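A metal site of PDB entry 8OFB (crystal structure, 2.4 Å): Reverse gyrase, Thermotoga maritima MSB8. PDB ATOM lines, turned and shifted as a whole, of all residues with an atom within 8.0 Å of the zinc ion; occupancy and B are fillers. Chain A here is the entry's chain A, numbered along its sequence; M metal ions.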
ATOM      1  N   SER A  10       4.530  16.961  -2.734  1.00  0.00           N
ATOM      2  CA  SER A  10       4.997  18.346  -2.756  1.00  0.00           C
ATOM      3  C   SER A  10       4.091  19.275  -3.553  1.00  0.00           C
ATOM      4  O   SER A  10       4.287  20.487  -3.504  1.00  0.00           O
ATOM      5  CB  SER A  10       6.425  18.414  -3.315  1.00  0.00           C
ATOM      6  OG  SER A  10       6.478  17.861  -4.623  1.00  0.00           O
ATOM      7  N   CYS A  11       3.121  18.736  -4.296  1.00  0.00           N
ATOM      8  CA  CYS A  11       2.201  19.593  -5.036  1.00  0.00           C
ATOM      9  C   CYS A  11       1.235  20.267  -4.080  1.00  0.00           C
ATOM     10  O   CYS A  11       0.633  19.620  -3.220  1.00  0.00           O
ATOM     11  CB  CYS A  11       1.435  18.786  -6.082  1.00  0.00           C
ATOM     12  SG  CYS A  11       0.244  19.776  -7.026  1.00  0.00           S
ATOM     13  N   ILE A  12       1.071  21.582  -4.242  1.00  0.00           N
ATOM     14  CA  ILE A  12       0.226  22.350  -3.338  1.00  0.00           C
ATOM     15  C   ILE A  12      -1.251  22.266  -3.679  1.00  0.00           C
ATOM     16  O   ILE A  12      -2.096  22.666  -2.867  1.00  0.00           O
ATOM     17  CB  ILE A  12       0.699  23.815  -3.318  1.00  0.00           C
ATOM     18  CG1 ILE A  12       0.231  24.531  -2.051  1.00  0.00           C
ATOM     19  CG2 ILE A  12       0.216  24.544  -4.566  1.00  0.00           C
ATOM     20  CD1 ILE A  12       0.701  25.964  -1.937  1.00  0.00           C
ATOM     21  N   ASN A  13      -1.601  21.731  -4.846  1.00  0.00           N
ATOM     22  CA  ASN A  13      -2.998  21.653  -5.280  1.00  0.00           C
ATOM     23  C   ASN A  13      -3.619  20.274  -5.081  1.00  0.00           C
ATOM     24  O   ASN A  13      -4.768  20.177  -4.657  1.00  0.00           O
ATOM     25  CB  ASN A  13      -3.121  22.051  -6.749  1.00  0.00           C
ATOM     26  CG  ASN A  13      -4.564  22.084  -7.228  1.00  0.00           C
ATOM     27  OD1 ASN A  13      -5.485  22.308  -6.442  1.00  0.00           O
ATOM     28  ND2 ASN A  13      -4.772  21.840  -8.513  1.00  0.00           N
ATOM     29  N   CYS A  14      -2.880  19.199  -5.376  1.00  0.00           N
ATOM     30  CA  CYS A  14      -3.417  17.853  -5.237  1.00  0.00           C
ATOM     31  C   CYS A  14      -2.638  16.987  -4.251  1.00  0.00           C
ATOM     32  O   CYS A  14      -3.071  15.858  -3.987  1.00  0.00           O
ATOM     33  CB  CYS A  14      -3.449  17.137  -6.598  1.00  0.00           C
ATOM     34  SG  CYS A  14      -1.834  16.662  -7.250  1.00  0.00           S
ATOM     35  N   GLY A  15      -1.522  17.459  -3.713  1.00  0.00           N
ATOM     36  CA  GLY A  15      -0.754  16.660  -2.786  1.00  0.00           C
ATOM     37  C   GLY A  15      -0.037  15.485  -3.402  1.00  0.00           C
ATOM     38  O   GLY A  15       0.309  14.538  -2.685  1.00  0.00           O
ATOM     39  N   GLY A  16       0.205  15.517  -4.708  1.00  0.00           N
ATOM     40  CA  GLY A  16       0.893  14.445  -5.394  1.00  0.00           C
ATOM     41  C   GLY A  16       2.356  14.789  -5.675  1.00  0.00           C
ATOM     42  O   GLY A  16       2.920  15.739  -5.149  1.00  0.00           O
ATOM     43  N   LEU A  17       2.956  13.972  -6.544  1.00  0.00           N
ATOM     44  CA  LEU A  17       4.340  14.175  -6.923  1.00  0.00           C
ATOM     45  C   LEU A  17       4.491  15.471  -7.716  1.00  0.00           C
ATOM     46  O   LEU A  17       3.643  15.818  -8.542  1.00  0.00           O
ATOM     47  CB  LEU A  17       4.843  12.987  -7.754  1.00  0.00           C
ATOM     48  CG  LEU A  17       6.341  12.928  -8.077  1.00  0.00           C
ATOM     49  CD1 LEU A  17       7.116  12.320  -6.918  1.00  0.00           C
ATOM     50  CD2 LEU A  17       6.590  12.162  -9.362  1.00  0.00           C
ATOM     51  N   ASN A  18       5.582  16.192  -7.467  1.00  0.00           N
ATOM     52  CA  ASN A  18       5.873  17.414  -8.190  1.00  0.00           C
ATOM     53  C   ASN A  18       7.387  17.605  -8.231  1.00  0.00           C
ATOM     54  O   ASN A  18       8.106  17.191  -7.328  1.00  0.00           O
ATOM     55  CB  ASN A  18       5.197  18.626  -7.545  1.00  0.00           C
ATOM     56  CG  ASN A  18       5.275  19.871  -8.419  1.00  0.00           C
ATOM     57  OD1 ASN A  18       5.572  19.793  -9.604  1.00  0.00           O
ATOM     58  ND2 ASN A  18       5.007  21.029  -7.822  1.00  0.00           N
ATOM     59  N   LEU A  27       4.608  26.806  -8.569  1.00  0.00           N
ATOM     60  CA  LEU A  27       3.627  26.137  -9.410  1.00  0.00           C
ATOM     61  C   LEU A  27       3.256  24.765  -8.847  1.00  0.00           C
ATOM     62  O   LEU A  27       4.063  24.125  -8.178  1.00  0.00           O
ATOM     63  CB  LEU A  27       4.166  25.968 -10.827  1.00  0.00           C
ATOM     64  CG  LEU A  27       4.673  27.231 -11.528  1.00  0.00           C
ATOM     65  CD1 LEU A  27       5.367  26.881 -12.823  1.00  0.00           C
ATOM     66  CD2 LEU A  27       3.529  28.205 -11.771  1.00  0.00           C
ATOM     67  N   PRO A  28       2.043  24.303  -9.115  1.00  0.00           N
ATOM     68  CA  PRO A  28       1.676  22.924  -8.786  1.00  0.00           C
ATOM     69  C   PRO A  28       2.253  21.967  -9.826  1.00  0.00           C
ATOM     70  O   PRO A  28       2.974  22.366 -10.738  1.00  0.00           O
ATOM     71  CB  PRO A  28       0.138  22.957  -8.834  1.00  0.00           C
ATOM     72  CG  PRO A  28      -0.175  24.025  -9.814  1.00  0.00           C
ATOM     73  CD  PRO A  28       0.894  25.076  -9.631  1.00  0.00           C
ATOM     74  N   CYS A  29       1.928  20.683  -9.673  1.00  0.00           N
ATOM     75  CA  CYS A  29       2.426  19.691 -10.607  1.00  0.00           C
ATOM     76  C   CYS A  29       1.781  19.882 -11.974  1.00  0.00           C
ATOM     77  O   CYS A  29       0.706  20.472 -12.109  1.00  0.00           O
ATOM     78  CB  CYS A  29       2.172  18.274 -10.093  1.00  0.00           C
ATOM     79  SG  CYS A  29       0.456  17.731 -10.161  1.00  0.00           S
ATOM     80  N   GLU A  30       2.460  19.377 -13.009  1.00  0.00           N
ATOM     81  CA  GLU A  30       2.005  19.580 -14.380  1.00  0.00           C
ATOM     82  C   GLU A  30       0.648  18.931 -14.651  1.00  0.00           C
ATOM     83  O   GLU A  30      -0.046  19.360 -15.577  1.00  0.00           O
ATOM     84  CB  GLU A  30       3.042  19.032 -15.364  1.00  0.00           C
ATOM     85  CG  GLU A  30       4.346  19.810 -15.379  1.00  0.00           C
ATOM     86  CD  GLU A  30       5.287  19.375 -16.485  1.00  0.00           C
ATOM     87  OE1 GLU A  30       4.906  18.484 -17.268  1.00  0.00           O
ATOM     88  OE2 GLU A  30       6.405  19.935 -16.568  1.00  0.00           O
ATOM     89  N   VAL A  31       0.268  17.925 -13.871  1.00  0.00           N
ATOM     90  CA  VAL A  31      -1.060  17.342 -14.020  1.00  0.00           C
ATOM     91  C   VAL A  31      -2.131  18.371 -13.702  1.00  0.00           C
ATOM     92  O   VAL A  31      -3.137  18.493 -14.410  1.00  0.00           O
ATOM     93  CB  VAL A  31      -1.207  16.087 -13.145  1.00  0.00           C
ATOM     94  CG1 VAL A  31      -2.547  15.417 -13.378  1.00  0.00           C
ATOM     95  CG2 VAL A  31      -0.061  15.119 -13.410  1.00  0.00           C
ATOM     96  N   CYS A  32      -1.936  19.130 -12.619  1.00  0.00           N
ATOM     97  CA  CYS A  32      -2.882  20.194 -12.284  1.00  0.00           C
ATOM     98  C   CYS A  32      -2.823  21.326 -13.295  1.00  0.00           C
ATOM     99  O   CYS A  32      -3.870  21.828 -13.737  1.00  0.00           O
ATOM    100  CB  CYS A  32      -2.592  20.734 -10.877  1.00  0.00           C
ATOM    101  SG  CYS A  32      -2.757  19.525  -9.544  1.00  0.00           S
ATOM    102  N   LEU A  33      -1.624  21.746 -13.702  1.00  0.00           N
ATOM    103  CA  LEU A  33      -1.445  22.895 -14.575  1.00  0.00           C
ATOM    104  C   LEU A  33      -0.219  22.665 -15.455  1.00  0.00           C
ATOM    105  O   LEU A  33       0.925  22.811 -15.001  1.00  0.00           O
ATOM    106  CB  LEU A  33      -1.306  24.192 -13.772  1.00  0.00           C
ATOM    107  CG  LEU A  33      -1.012  25.462 -14.561  1.00  0.00           C
ATOM    108  CD1 LEU A  33      -2.096  25.715 -15.593  1.00  0.00           C
ATOM    109  CD2 LEU A  33      -0.892  26.651 -13.616  1.00  0.00           C
ATOM    110  N   LEU A  45      -6.372  26.852 -12.376  1.00  0.00           N
ATOM    111  CA  LEU A  45      -6.915  25.604 -11.874  1.00  0.00           C
ATOM    112  C   LEU A  45      -8.440  25.578 -11.979  1.00  0.00           C
ATOM    113  O   LEU A  45      -9.032  24.517 -12.237  1.00  0.00           O
ATOM    114  CB  LEU A  45      -6.472  25.382 -10.435  1.00  0.00           C
ATOM    115  CG  LEU A  45      -4.958  25.305 -10.239  1.00  0.00           C
ATOM    116  CD1 LEU A  45      -4.601  25.230  -8.760  1.00  0.00           C
ATOM    117  CD2 LEU A  45      -4.377  24.128 -10.996  1.00  0.00           C
ATOM    118  N   THR A  50      -9.261  21.453 -12.178  1.00  0.00           N
ATOM    119  CA  THR A  50      -8.361  20.638 -11.372  1.00  0.00           C
ATOM    120  C   THR A  50      -8.140  21.226  -9.988  1.00  0.00           C
ATOM    121  O   THR A  50      -7.279  20.748  -9.245  1.00  0.00           O
ATOM    122  CB  THR A  50      -7.017  20.465 -12.085  1.00  0.00           C
ATOM    123  OG1 THR A  50      -6.418  21.747 -12.304  1.00  0.00           O
ATOM    124  CG2 THR A  50      -7.217  19.761 -13.425  1.00  0.00           C
ATOM    125  N   LYS A  52      -8.284  21.521  -6.413  1.00  0.00           N
ATOM    126  CA  LYS A  52      -8.612  20.633  -5.304  1.00  0.00           C
ATOM    127  C   LYS A  52      -8.276  21.245  -3.953  1.00  0.00           C
ATOM    128  O   LYS A  52      -9.168  21.369  -3.112  1.00  0.00           O
ATOM    129  CB  LYS A  52      -7.900  19.283  -5.486  1.00  0.00           C
ATOM    130  CG  LYS A  52      -8.268  18.548  -6.754  1.00  0.00           C
ATOM    131  CD  LYS A  52      -7.496  17.251  -6.886  1.00  0.00           C
ATOM    132  CE  LYS A  52      -7.826  16.534  -8.183  1.00  0.00           C
ATOM    133  NZ  LYS A  52      -7.055  15.261  -8.314  1.00  0.00           N
HETATM  134 ZN    ZN M   1      -0.981  18.445  -8.482  1.00  0.00          ZN
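SG of Cys 32 lies close to ND2 of Asn 13, at 3.2 Å. N of Gly 16 sits close to SG of Cys 14 (3.5 Å). The backbone carbonyl oxygen (O) of Cys 32 lies within hydrogen-bond range of the side-chain hydroxyl (OG1) of Thr 50, at 2.9 Å. The side-chain sulfur of Cys 11 lies close to the backbone NH of Asn 13 (3.5 Å). The backbone NH (N) of Cys 11 sits at hydrogen-bond distance from the backbone carbonyl oxygen (O) of Gly 16 (3.1 Å). The backbone NH (N) of Val 31 sits close to the side-chain sulfur (SG) of Cys 29 (3.7 Å).
The zinc ion is bound by SG of Cys 29 (2.3 Å). SG of Cys 11 binds the zinc ion, at 2.3 Å. SG of Cys 14 is bound to the zinc ion (2.3 Å). The zinc ion is bound by SG of Cys 32 (2.3 Å). The zinc ion has four donor atoms within binding distance.
Within 4 Å of the zinc ion: Cys 11, Cys 14, Cys 29 and Cys 32.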
